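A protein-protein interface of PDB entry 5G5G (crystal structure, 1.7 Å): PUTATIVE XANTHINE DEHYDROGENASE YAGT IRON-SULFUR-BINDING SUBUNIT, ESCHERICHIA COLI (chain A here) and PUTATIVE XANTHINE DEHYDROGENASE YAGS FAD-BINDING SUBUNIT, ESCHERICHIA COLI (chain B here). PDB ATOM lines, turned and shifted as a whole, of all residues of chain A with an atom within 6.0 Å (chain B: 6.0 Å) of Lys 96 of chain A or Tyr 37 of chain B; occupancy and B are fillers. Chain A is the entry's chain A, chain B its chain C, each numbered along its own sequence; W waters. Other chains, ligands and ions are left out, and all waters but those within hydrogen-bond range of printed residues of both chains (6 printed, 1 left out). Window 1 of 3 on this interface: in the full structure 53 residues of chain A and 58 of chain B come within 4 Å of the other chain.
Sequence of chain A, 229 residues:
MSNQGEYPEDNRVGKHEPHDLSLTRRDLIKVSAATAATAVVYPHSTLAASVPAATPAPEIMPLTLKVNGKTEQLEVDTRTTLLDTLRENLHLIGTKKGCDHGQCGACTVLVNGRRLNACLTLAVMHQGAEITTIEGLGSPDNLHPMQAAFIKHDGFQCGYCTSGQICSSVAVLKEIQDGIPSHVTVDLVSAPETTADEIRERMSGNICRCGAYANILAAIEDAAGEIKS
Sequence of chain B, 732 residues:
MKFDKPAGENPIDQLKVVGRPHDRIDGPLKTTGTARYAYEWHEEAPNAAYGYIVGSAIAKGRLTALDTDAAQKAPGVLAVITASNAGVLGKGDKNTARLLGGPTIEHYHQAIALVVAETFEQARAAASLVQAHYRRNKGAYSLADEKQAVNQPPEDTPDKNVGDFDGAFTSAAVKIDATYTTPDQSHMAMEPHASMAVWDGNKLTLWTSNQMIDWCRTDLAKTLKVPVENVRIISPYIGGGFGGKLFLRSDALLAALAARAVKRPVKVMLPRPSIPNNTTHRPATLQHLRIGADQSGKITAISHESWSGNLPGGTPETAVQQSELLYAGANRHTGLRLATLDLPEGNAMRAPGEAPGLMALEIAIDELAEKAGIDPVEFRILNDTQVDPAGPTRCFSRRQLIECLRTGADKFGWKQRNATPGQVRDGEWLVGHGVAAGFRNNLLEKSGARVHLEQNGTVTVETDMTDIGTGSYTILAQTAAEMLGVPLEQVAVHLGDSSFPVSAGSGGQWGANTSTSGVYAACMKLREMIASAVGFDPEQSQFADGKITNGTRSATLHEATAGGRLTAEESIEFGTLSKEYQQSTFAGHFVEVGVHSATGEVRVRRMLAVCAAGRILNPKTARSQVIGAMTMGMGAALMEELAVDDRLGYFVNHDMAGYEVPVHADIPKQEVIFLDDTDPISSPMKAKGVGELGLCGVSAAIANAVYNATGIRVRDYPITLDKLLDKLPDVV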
ATOM      1  N   LEU A  83      10.755  20.832 -14.049  1.00  0.00           N
ATOM      2  CA  LEU A  83      11.358  20.112 -15.168  1.00  0.00           C
ATOM      3  C   LEU A  83      11.024  20.673 -16.545  1.00  0.00           C
ATOM      4  O   LEU A  83      11.872  20.962 -17.351  1.00  0.00           O
ATOM      5  CB  LEU A  83      10.944  18.632 -15.110  1.00  0.00           C
ATOM      6  CG  LEU A  83      11.405  17.737 -16.258  1.00  0.00           C
ATOM      7  CD1 LEU A  83      12.927  17.768 -16.326  1.00  0.00           C
ATOM      8  CD2 LEU A  83      10.907  16.325 -16.001  1.00  0.00           C
ATOM      9  N   ARG A  87      13.333  22.644 -19.351  1.00  0.00           N
ATOM     10  CA  ARG A  87      13.453  22.090 -20.709  1.00  0.00           C
ATOM     11  C   ARG A  87      12.769  22.912 -21.837  1.00  0.00           C
ATOM     12  O   ARG A  87      13.397  23.268 -22.845  1.00  0.00           O
ATOM     13  CB  ARG A  87      12.967  20.645 -20.717  1.00  0.00           C
ATOM     14  CG  ARG A  87      13.910  19.693 -20.008  1.00  0.00           C
ATOM     15  CD  ARG A  87      13.221  18.378 -19.694  1.00  0.00           C
ATOM     16  NE  ARG A  87      12.758  17.639 -20.889  1.00  0.00           N
ATOM     17  CZ  ARG A  87      13.527  16.940 -21.712  1.00  0.00           C
ATOM     18  NH1 ARG A  87      14.846  16.859 -21.507  1.00  0.00           N
ATOM     19  NH2 ARG A  87      12.967  16.292 -22.737  1.00  0.00           N
ATOM     20  N   ILE A  93      18.114  21.767 -21.710  1.00  0.00           N
ATOM     21  CA  ILE A  93      17.658  20.429 -22.003  1.00  0.00           C
ATOM     22  C   ILE A  93      18.507  19.331 -21.325  1.00  0.00           C
ATOM     23  O   ILE A  93      18.215  18.137 -21.481  1.00  0.00           O
ATOM     24  CB  ILE A  93      17.490  20.204 -23.542  1.00  0.00           C
ATOM     25  CG1 ILE A  93      18.792  20.497 -24.309  1.00  0.00           C
ATOM     26  CG2 ILE A  93      16.262  20.982 -24.098  1.00  0.00           C
ATOM     27  CD1 ILE A  93      19.929  19.512 -24.008  1.00  0.00           C
ATOM     28  N   GLY A  94      19.505  19.711 -20.523  1.00  0.00           N
ATOM     29  CA  GLY A  94      20.346  18.717 -19.852  1.00  0.00           C
ATOM     30  C   GLY A  94      19.615  17.883 -18.803  1.00  0.00           C
ATOM     31  O   GLY A  94      19.882  16.710 -18.639  1.00  0.00           O
ATOM     32  N   THR A  95      18.649  18.488 -18.114  1.00  0.00           N
ATOM     33  CA  THR A  95      17.771  17.801 -17.195  1.00  0.00           C
ATOM     34  C   THR A  95      16.777  16.972 -18.025  1.00  0.00           C
ATOM     35  O   THR A  95      16.180  17.459 -18.964  1.00  0.00           O
ATOM     36  CB  THR A  95      17.030  18.815 -16.293  1.00  0.00           C
ATOM     37  OG1 THR A  95      17.980  19.684 -15.634  1.00  0.00           O
ATOM     38  CG2 THR A  95      16.217  18.117 -15.265  1.00  0.00           C
ATOM     39  N   LYS A  96      16.659  15.691 -17.698  1.00  0.00           N
ATOM     40  CA  LYS A  96      15.889  14.772 -18.548  1.00  0.00           C
ATOM     41  C   LYS A  96      14.574  14.385 -17.948  1.00  0.00           C
ATOM     42  O   LYS A  96      14.376  14.488 -16.758  1.00  0.00           O
ATOM     43  CB  LYS A  96      16.705  13.503 -18.814  1.00  0.00           C
ATOM     44  CG  LYS A  96      18.063  13.752 -19.426  1.00  0.00           C
ATOM     45  CD  LYS A  96      18.006  14.639 -20.673  1.00  0.00           C
ATOM     46  CE  LYS A  96      19.354  14.706 -21.398  1.00  0.00           C
ATOM     47  NZ  LYS A  96      19.394  15.815 -22.411  1.00  0.00           N
ATOM     48  N   LYS A  97      13.689  13.884 -18.803  1.00  0.00           N
ATOM     49  CA  LYS A  97      12.387  13.339 -18.392  1.00  0.00           C
ATOM     50  C   LYS A  97      12.333  11.860 -18.703  1.00  0.00           C
ATOM     51  O   LYS A  97      12.155  11.481 -19.836  1.00  0.00           O
ATOM     52  CB  LYS A  97      11.238  14.051 -19.126  1.00  0.00           C
ATOM     53  CG  LYS A  97       9.852  13.568 -18.706  1.00  0.00           C
ATOM     54  CD  LYS A  97       8.666  14.285 -19.352  1.00  0.00           C
ATOM     55  CE  LYS A  97       8.436  15.709 -18.907  1.00  0.00           C
ATOM     56  NZ  LYS A  97       7.118  16.220 -19.462  1.00  0.00           N
ATOM     57  N   GLY A  98      12.479  11.038 -17.682  1.00  0.00           N
ATOM     58  CA  GLY A  98      12.428   9.572 -17.848  1.00  0.00           C
ATOM     59  C   GLY A  98      11.094   8.941 -17.530  1.00  0.00           C
ATOM     60  O   GLY A  98      10.843   7.804 -17.975  1.00  0.00           O
ATOM     61  N   ALA A 106      15.798  10.876 -13.320  1.00  0.00           N
ATOM     62  CA  ALA A 106      16.507  11.457 -14.461  1.00  0.00           C
ATOM     63  C   ALA A 106      16.410  12.997 -14.517  1.00  0.00           C
ATOM     64  O   ALA A 106      17.241  13.660 -15.140  1.00  0.00           O
ATOM     65  CB  ALA A 106      16.014  10.862 -15.760  1.00  0.00           C
ATOM     66  N   CYS A 107      15.408  13.535 -13.801  1.00  0.00           N
ATOM     67  CA  CYS A 107      15.130  14.967 -13.734  1.00  0.00           C
ATOM     68  C   CYS A 107      15.738  15.590 -12.470  1.00  0.00           C
ATOM     69  O   CYS A 107      15.328  16.681 -12.073  1.00  0.00           O
ATOM     70  CB  CYS A 107      13.576  15.088 -13.690  1.00  0.00           C
ATOM     71  SG  CYS A 107      12.917  14.381 -12.163  1.00  0.00           S
ATOM     72  N   THR A 108      16.719  14.951 -11.830  1.00  0.00           N
ATOM     73  CA  THR A 108      17.239  15.501 -10.567  1.00  0.00           C
ATOM     74  C   THR A 108      17.937  16.861 -10.824  1.00  0.00           C
ATOM     75  O   THR A 108      18.755  16.969 -11.763  1.00  0.00           O
ATOM     76  CB  THR A 108      18.253  14.559  -9.924  1.00  0.00           C
ATOM     77  OG1 THR A 108      17.635  13.273  -9.684  1.00  0.00           O
ATOM     78  CG2 THR A 108      18.864  15.127  -8.631  1.00  0.00           C
ATOM     79  N   CYS A 158      24.147   5.127 -22.447  1.00  0.00           N
ATOM     80  CA  CYS A 158      23.257   5.897 -23.302  1.00  0.00           C
ATOM     81  C   CYS A 158      23.280   7.380 -22.979  1.00  0.00           C
ATOM     82  O   CYS A 158      22.977   8.173 -23.863  1.00  0.00           O
ATOM     83  CB  CYS A 158      21.828   5.391 -23.269  1.00  0.00           C
ATOM     84  SG  CYS A 158      20.812   5.939 -21.906  1.00  0.00           S
ATOM     85  N   GLY A 159      23.630   7.732 -21.740  1.00  0.00           N
ATOM     86  CA  GLY A 159      23.740   9.105 -21.328  1.00  0.00           C
ATOM     87  C   GLY A 159      22.440   9.733 -20.806  1.00  0.00           C
ATOM     88  O   GLY A 159      22.478  10.888 -20.371  1.00  0.00           O
ATOM     89  N   TYR A 160      21.328   9.021 -20.826  1.00  0.00           N
ATOM     90  CA  TYR A 160      20.042   9.669 -20.527  1.00  0.00           C
ATOM     91  C   TYR A 160      19.827   9.848 -19.012  1.00  0.00           C
ATOM     92  O   TYR A 160      19.188  10.791 -18.606  1.00  0.00           O
ATOM     93  CB  TYR A 160      18.894   8.979 -21.245  1.00  0.00           C
ATOM     94  CG  TYR A 160      17.666   9.846 -21.373  1.00  0.00           C
ATOM     95  CD1 TYR A 160      17.623  10.887 -22.308  1.00  0.00           C
ATOM     96  CD2 TYR A 160      16.581   9.674 -20.536  1.00  0.00           C
ATOM     97  CE1 TYR A 160      16.555  11.718 -22.403  1.00  0.00           C
ATOM     98  CE2 TYR A 160      15.486  10.509 -20.628  1.00  0.00           C
ATOM     99  CZ  TYR A 160      15.466  11.515 -21.569  1.00  0.00           C
ATOM    100  OH  TYR A 160      14.408  12.396 -21.722  1.00  0.00           O
ATOM    101  N   CYS A 161      20.324   8.933 -18.167  1.00  0.00           N
ATOM    102  CA  CYS A 161      20.217   9.096 -16.702  1.00  0.00           C
ATOM    103  C   CYS A 161      21.352   9.904 -16.140  1.00  0.00           C
ATOM    104  O   CYS A 161      21.365  10.223 -14.953  1.00  0.00           O
ATOM    105  CB  CYS A 161      20.178   7.725 -16.032  1.00  0.00           C
ATOM    106  SG  CYS A 161      21.760   6.882 -15.823  1.00  0.00           S
ATOM    107  N   SER A 163      22.750  13.040 -16.409  1.00  0.00           N
ATOM    108  CA  SER A 163      22.589  14.341 -15.773  1.00  0.00           C
ATOM    109  C   SER A 163      22.112  14.178 -14.333  1.00  0.00           C
ATOM    110  O   SER A 163      22.621  14.814 -13.419  1.00  0.00           O
ATOM    111  CB  SER A 163      21.606  15.231 -16.546  1.00  0.00           C
ATOM    112  OG  SER A 163      22.121  15.472 -17.852  1.00  0.00           O
ATOM    113  N   LYS B  30      27.694  13.937 -23.043  1.00  0.00           N
ATOM    114  CA  LYS B  30      26.718  13.216 -22.290  1.00  0.00           C
ATOM    115  C   LYS B  30      26.763  13.524 -20.785  1.00  0.00           C
ATOM    116  O   LYS B  30      25.762  13.318 -20.118  1.00  0.00           O
ATOM    117  CB  LYS B  30      26.808  11.697 -22.518  1.00  0.00           C
ATOM    118  CG  LYS B  30      26.246  11.285 -23.864  1.00  0.00           C
ATOM    119  CD  LYS B  30      26.368   9.787 -24.040  1.00  0.00           C
ATOM    120  CE  LYS B  30      25.678   9.362 -25.311  1.00  0.00           C
ATOM    121  NZ  LYS B  30      25.686   7.886 -25.514  1.00  0.00           N
ATOM    122  N   GLY B  33      25.053  17.413 -20.116  1.00  0.00           N
ATOM    123  CA  GLY B  33      23.664  17.688 -20.581  1.00  0.00           C
ATOM    124  C   GLY B  33      23.617  18.430 -21.908  1.00  0.00           C
ATOM    125  O   GLY B  33      22.693  19.239 -22.176  1.00  0.00           O
ATOM    126  N   THR B  34      24.612  18.185 -22.758  1.00  0.00           N
ATOM    127  CA  THR B  34      24.641  18.856 -24.055  1.00  0.00           C
ATOM    128  C   THR B  34      24.440  17.962 -25.260  1.00  0.00           C
ATOM    129  O   THR B  34      24.329  18.487 -26.364  1.00  0.00           O
ATOM    130  CB  THR B  34      25.847  19.764 -24.210  1.00  0.00           C
ATOM    131  OG1 THR B  34      27.062  19.060 -23.976  1.00  0.00           O
ATOM    132  CG2 THR B  34      25.737  20.975 -23.244  1.00  0.00           C
ATOM    133  N   ALA B  35      24.338  16.640 -25.061  1.00  0.00           N
ATOM    134  CA  ALA B  35      23.947  15.745 -26.138  1.00  0.00           C
ATOM    135  C   ALA B  35      22.438  15.939 -26.323  1.00  0.00           C
ATOM    136  O   ALA B  35      21.707  15.821 -25.331  1.00  0.00           O
ATOM    137  CB  ALA B  35      24.230  14.298 -25.722  1.00  0.00           C
ATOM    138  N   ARG B  36      21.973  16.135 -27.549  1.00  0.00           N
ATOM    139  CA  ARG B  36      20.513  16.274 -27.783  1.00  0.00           C
ATOM    140  C   ARG B  36      19.865  14.962 -28.137  1.00  0.00           C
ATOM    141  O   ARG B  36      20.231  14.300 -29.118  1.00  0.00           O
ATOM    142  CB  ARG B  36      20.210  17.264 -28.888  1.00  0.00           C
ATOM    143  CG  ARG B  36      20.758  18.674 -28.740  1.00  0.00           C
ATOM    144  CD  ARG B  36      20.307  19.388 -27.527  1.00  0.00           C
ATOM    145  NE  ARG B  36      20.896  20.742 -27.571  1.00  0.00           N
ATOM    146  CZ  ARG B  36      20.395  21.789 -28.222  1.00  0.00           C
ATOM    147  NH1 ARG B  36      19.161  21.758 -28.732  1.00  0.00           N
ATOM    148  NH2 ARG B  36      21.110  22.937 -28.280  1.00  0.00           N
ATOM    149  N   TYR B  37      18.798  14.683 -27.421  1.00  0.00           N
ATOM    150  CA  TYR B  37      17.869  13.589 -27.710  1.00  0.00           C
ATOM    151  C   TYR B  37      16.645  14.156 -28.455  1.00  0.00           C
ATOM    152  O   TYR B  37      16.476  15.360 -28.574  1.00  0.00           O
ATOM    153  CB  TYR B  37      17.519  12.893 -26.374  1.00  0.00           C
ATOM    154  CG  TYR B  37      18.748  12.279 -25.679  1.00  0.00           C
ATOM    155  CD1 TYR B  37      19.555  13.048 -24.864  1.00  0.00           C
ATOM    156  CD2 TYR B  37      19.078  10.935 -25.853  1.00  0.00           C
ATOM    157  CE1 TYR B  37      20.698  12.566 -24.280  1.00  0.00           C
ATOM    158  CE2 TYR B  37      20.224  10.409 -25.266  1.00  0.00           C
ATOM    159  CZ  TYR B  37      21.008  11.211 -24.457  1.00  0.00           C
ATOM    160  OH  TYR B  37      22.182  10.749 -23.847  1.00  0.00           O
ATOM    161  N   ALA B  38      15.824  13.254 -28.989  1.00  0.00           N
ATOM    162  CA  ALA B  38      14.751  13.551 -29.948  1.00  0.00           C
ATOM    163  C   ALA B  38      13.822  14.692 -29.550  1.00  0.00           C
ATOM    164  O   ALA B  38      13.429  15.440 -30.391  1.00  0.00           O
ATOM    165  CB  ALA B  38      13.941  12.312 -30.214  1.00  0.00           C
ATOM    166  N   TYR B  39      13.537  14.847 -28.269  1.00  0.00           N
ATOM    167  CA  TYR B  39      12.561  15.864 -27.840  1.00  0.00           C
ATOM    168  C   TYR B  39      13.244  17.194 -27.493  1.00  0.00           C
ATOM    169  O   TYR B  39      12.596  18.084 -26.937  1.00  0.00           O
ATOM    170  CB  TYR B  39      11.860  15.375 -26.603  1.00  0.00           C
ATOM    171  CG  TYR B  39      10.444  15.878 -26.318  1.00  0.00           C
ATOM    172  CD1 TYR B  39       9.343  15.369 -27.036  1.00  0.00           C
ATOM    173  CD2 TYR B  39      10.211  16.771 -25.248  1.00  0.00           C
ATOM    174  CE1 TYR B  39       8.026  15.786 -26.713  1.00  0.00           C
ATOM    175  CE2 TYR B  39       8.926  17.189 -24.956  1.00  0.00           C
ATOM    176  CZ  TYR B  39       7.857  16.678 -25.655  1.00  0.00           C
ATOM    177  OH  TYR B  39       6.544  17.036 -25.337  1.00  0.00           O
ATOM    178  N   GLU B  40      14.523  17.324 -27.827  1.00  0.00           N
ATOM    179  CA  GLU B  40      15.360  18.439 -27.338  1.00  0.00           C
ATOM    180  C   GLU B  40      15.943  19.343 -28.425  1.00  0.00           C
ATOM    181  O   GLU B  40      16.850  20.125 -28.152  1.00  0.00           O
ATOM    182  CB  GLU B  40      16.482  17.828 -26.483  1.00  0.00           C
ATOM    183  CG  GLU B  40      15.913  17.036 -25.308  1.00  0.00           C
ATOM    184  CD  GLU B  40      16.951  16.196 -24.565  1.00  0.00           C
ATOM    185  OE1 GLU B  40      18.138  16.212 -24.959  1.00  0.00           O
ATOM    186  OE2 GLU B  40      16.577  15.572 -23.573  1.00  0.00           O
ATOM    187  N   TRP B  41      15.490  19.193 -29.665  1.00  0.00           N
ATOM    188  CA  TRP B  41      16.026  19.927 -30.809  1.00  0.00           C
ATOM    189  C   TRP B  41      15.307  21.292 -31.013  1.00  0.00           C
ATOM    190  O   TRP B  41      14.738  21.566 -32.075  1.00  0.00           O
ATOM    191  CB  TRP B  41      15.872  19.082 -32.072  1.00  0.00           C
ATOM    192  CG  TRP B  41      16.698  17.795 -32.054  1.00  0.00           C
ATOM    193  CD1 TRP B  41      16.226  16.526 -31.917  1.00  0.00           C
ATOM    194  CD2 TRP B  41      18.121  17.674 -32.203  1.00  0.00           C
ATOM    195  NE1 TRP B  41      17.262  15.620 -31.969  1.00  0.00           N
ATOM    196  CE2 TRP B  41      18.425  16.292 -32.177  1.00  0.00           C
ATOM    197  CE3 TRP B  41      19.162  18.595 -32.430  1.00  0.00           C
ATOM    198  CZ2 TRP B  41      19.724  15.811 -32.310  1.00  0.00           C
ATOM    199  CZ3 TRP B  41      20.459  18.128 -32.540  1.00  0.00           C
ATOM    200  CH2 TRP B  41      20.727  16.735 -32.490  1.00  0.00           C
ATOM    201  N   GLU B 191      15.092   6.768 -21.871  1.00  0.00           N
ATOM    202  CA  GLU B 191      14.454   7.778 -22.731  1.00  0.00           C
ATOM    203  C   GLU B 191      13.147   7.225 -23.268  1.00  0.00           C
ATOM    204  O   GLU B 191      13.153   6.276 -24.047  1.00  0.00           O
ATOM    205  CB  GLU B 191      15.389   8.234 -23.880  1.00  0.00           C
ATOM    206  CG  GLU B 191      14.771   9.269 -24.825  1.00  0.00           C
ATOM    207  CD  GLU B 191      15.456   9.330 -26.192  1.00  0.00           C
ATOM    208  OE1 GLU B 191      16.190   8.375 -26.578  1.00  0.00           O
ATOM    209  OE2 GLU B 191      15.232  10.340 -26.880  1.00  0.00           O
ATOM    210  N   THR B 208      14.329  11.498 -34.096  1.00  0.00           N
ATOM    211  CA  THR B 208      13.673  10.406 -33.394  1.00  0.00           C
ATOM    212  C   THR B 208      14.673   9.653 -32.529  1.00  0.00           C
ATOM    213  O   THR B 208      15.855  10.045 -32.440  1.00  0.00           O
ATOM    214  CB  THR B 208      12.968   9.461 -34.436  1.00  0.00           C
ATOM    215  OG1 THR B 208      12.083   8.523 -33.791  1.00  0.00           O
ATOM    216  CG2 THR B 208      14.005   8.730 -35.254  1.00  0.00           C
ATOM    217  N   TYR B 237      21.774  10.581 -30.909  1.00  0.00           N
ATOM    218  CA  TYR B 237      21.817  10.129 -29.504  1.00  0.00           C
ATOM    219  C   TYR B 237      20.504   9.476 -29.106  1.00  0.00           C
ATOM    220  O   TYR B 237      19.430  10.049 -29.319  1.00  0.00           O
ATOM    221  CB  TYR B 237      22.161  11.271 -28.525  1.00  0.00           C
ATOM    222  CG  TYR B 237      23.485  11.868 -28.843  1.00  0.00           C
ATOM    223  CD1 TYR B 237      24.645  11.203 -28.517  1.00  0.00           C
ATOM    224  CD2 TYR B 237      23.572  13.060 -29.575  1.00  0.00           C
ATOM    225  CE1 TYR B 237      25.886  11.714 -28.878  1.00  0.00           C
ATOM    226  CE2 TYR B 237      24.806  13.556 -29.951  1.00  0.00           C
ATOM    227  CZ  TYR B 237      25.941  12.859 -29.598  1.00  0.00           C
ATOM    228  OH  TYR B 237      27.141  13.364 -29.975  1.00  0.00           O
ATOM    229  N   ILE B 238      20.596   8.271 -28.550  1.00  0.00           N
ATOM    230  CA  ILE B 238      19.439   7.434 -28.197  1.00  0.00           C
ATOM    231  C   ILE B 238      19.641   7.038 -26.747  1.00  0.00           C
ATOM    232  O   ILE B 238      20.700   6.504 -26.393  1.00  0.00           O
ATOM    233  CB  ILE B 238      19.381   6.185 -29.060  1.00  0.00           C
ATOM    234  CG1 ILE B 238      19.076   6.598 -30.485  1.00  0.00           C
ATOM    235  CG2 ILE B 238      18.330   5.173 -28.563  1.00  0.00           C
ATOM    236  CD1 ILE B 238      19.986   6.069 -31.497  1.00  0.00           C
ATOM    237  N   GLY B 239      18.656   7.328 -25.914  1.00  0.00           N
ATOM    238  CA  GLY B 239      18.707   7.054 -24.531  1.00  0.00           C
ATOM    239  C   GLY B 239      18.295   5.625 -24.243  1.00  0.00           C
ATOM    240  O   GLY B 239      17.409   5.377 -23.402  1.00  0.00           O
ATOM    241  N   GLY B 240      19.014   4.668 -24.847  1.00  0.00           N
ATOM    242  CA  GLY B 240      18.732   3.262 -24.628  1.00  0.00           C
ATOM    243  C   GLY B 240      17.623   2.747 -25.513  1.00  0.00           C
ATOM    244  O   GLY B 240      16.729   3.499 -25.924  1.00  0.00           O
HETATM  245  O   HOH W   1      22.231  15.649 -22.701  1.00  0.00           O
HETATM  246  O   HOH W   2      14.435  14.046 -23.830  1.00  0.00           O
HETATM  247  O   HOH W   3      24.564  15.030 -18.591  1.00  0.00           O
HETATM  248  O   HOH W   4      23.321   7.412 -27.129  1.00  0.00           O
HETATM  249  O   HOH W   5      23.340  13.249 -21.692  1.00  0.00           O
HETATM  250  O   HOH W   6       7.116  15.731 -22.194  1.00  0.00           O
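Water W3 lies within hydrogen-bond range of the backbone carbonyl oxygen (O) of Lys 30 of chain B (2.6 Å), the side-chain hydroxyl (OG) of Ser 163 of chain A (2.6 Å) and the backbone NH (N) of Gly 33 of chain B (2.9 Å). Water W2 lies within hydrogen-bond range of the side-chain carboxylate of Glu 40 of chain B, the side-chain hydroxyl of Tyr 160 of chain A and the guanidinium group of Arg 87 of chain A. Water W1 lies within hydrogen-bond range of the backbone carbonyl oxygen of Ala 35 of chain B (2.7 Å), the side-chain amino group of Lys 96 of chain A (2.9 Å) and the backbone NH of Thr 34 of chain B (3.5 Å). Water W6 bridges the side-chain amino group of Lys 97 of chain A and the side-chain hydroxyl of Tyr 39 of chain B. Water W5 lies within hydrogen-bond range of the backbone carbonyl oxygen (O) of Gly 159 of chain A (2.8 Å), the backbone carbonyl oxygen (O) of Lys 30 of chain B (2.9 Å) and the side-chain hydroxyl (OH) of Tyr 37 of chain B (3.5 Å). Water W4 lies within hydrogen-bond range of O of Ile 238 of chain B, NZ of Lys 30 of chain B and O of Cys 158 of chain A.
Of chain B, only Ala 35, Tyr 37 and Glu 40 come within 4 Å of Lys 96 of chain A. Tyr 37 of chain B touches just these residues of chain A: Lys 96, Cys 158, Gly 159 and Tyr 160. Of the printed residues of chain B, Gly 94 of chain A touches Gly 33 (3.3 Å). Printed residues of chain A within 4 Å of Ala 35 of chain B: Lys 96. Of the printed residues of chain B, Cys 158 of chain A touches Lys 30, Tyr 37, Ile 238, Gly 239 and Gly 240. Cys 107 of chain A touches none of the printed residues of chain B. Gly 98 of chain A touches none of the printed residues of chain B. The nearest residue of chain B that does not touch Lys 96 of chain A is Gly 33 of chain B (4.8 Å). The nearest printed residue of chain A that does not touch Ala 35 of chain B is Ile 93 of chain A (4.3 Å).
The side-chain sulfur (SG) of Cys 158 of chain A sits close to the backbone carbonyl oxygen (O) of Gly 239 of chain B, at 3.8 Å. The backbone NH of Gly 240 of chain B lies close to the side-chain sulfur of Cys 158 of chain A. OE2 of Glu 40 of chain B lies within salt-bridge range of NH1 of Arg 87 of chain A. The backbone carbonyl oxygen of Gly 159 of chain A sits close to the side-chain hydroxyl of Tyr 37 of chain B (3.5 Å). The backbone carbonyl oxygen (O) of Cys 158 of chain A is in hydrogen-bond range of the side-chain hydroxyl (OH) of Tyr 37 of chain B, 2.7 Å away. The backbone carbonyl oxygen (O) of Cys 158 of chain A sits at hydrogen-bond distance from the side-chain amino group (NZ) of Lys 30 of chain B (3.2 Å). NZ of Lys 96 of chain A lies within salt-bridge range of OE1 of Glu 40 of chain B.
Hydrophobic or aromatic side chains of chain B within 4 Å of the printed part of chain A: Tyr 37 and Tyr 39. Among the printed residues, 20 pairs touch across the chains.
Among the printed residues, pairs that only touch across the chains: Arg 87 of chain A with Tyr 39 of chain B, Ile 93 of chain A with Gly 33 of chain B, Ile 93 of chain A with Arg 36 of chain B, Ile 93 of chain A with Glu 40 of chain B, Gly 94 of chain A with Gly 33 of chain B, Lys 96 of chain A with Ala 35 of chain B, Lys 96 of chain A with Tyr 37 of chain B, Cys 158 of chain A with Ile 238 of chain B, Gly 159 of chain A with Lys 30 of chain B, Tyr 160 of chain A with Tyr 37 of chain B, Tyr 160 of chain A with Glu 191 of chain B, Tyr 160 of chain A with Gly 239 of chain B and Ser 163 of chain A with Gly 33 of chain B.
The backbone NH (N) of Lys 96 of chain A sits at hydrogen-bond distance from the backbone carbonyl oxygen (O) of Ala 106 of chain A, at 3.3 Å. NH1 of Arg 87 of chain A lies within hydrogen-bond range of O of Thr 95 of chain A. The side-chain hydroxyl (OH) of Tyr 160 of chain A is in hydrogen-bond range of the backbone carbonyl oxygen (O) of Lys 97 of chain A (3.1 Å). The backbone carbonyl oxygen of Glu 40 of chain B is in hydrogen-bond range of the guanidinium group of Arg 36 of chain B (2.9 Å). The side-chain sulfur of Cys 158 of chain A sits close to the backbone NH of Tyr 160 of chain A, 3.3 Å away. O of Tyr 37 of chain B is in hydrogen-bond range of NE1 of Trp 41 of chain B, at 3.5 Å.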
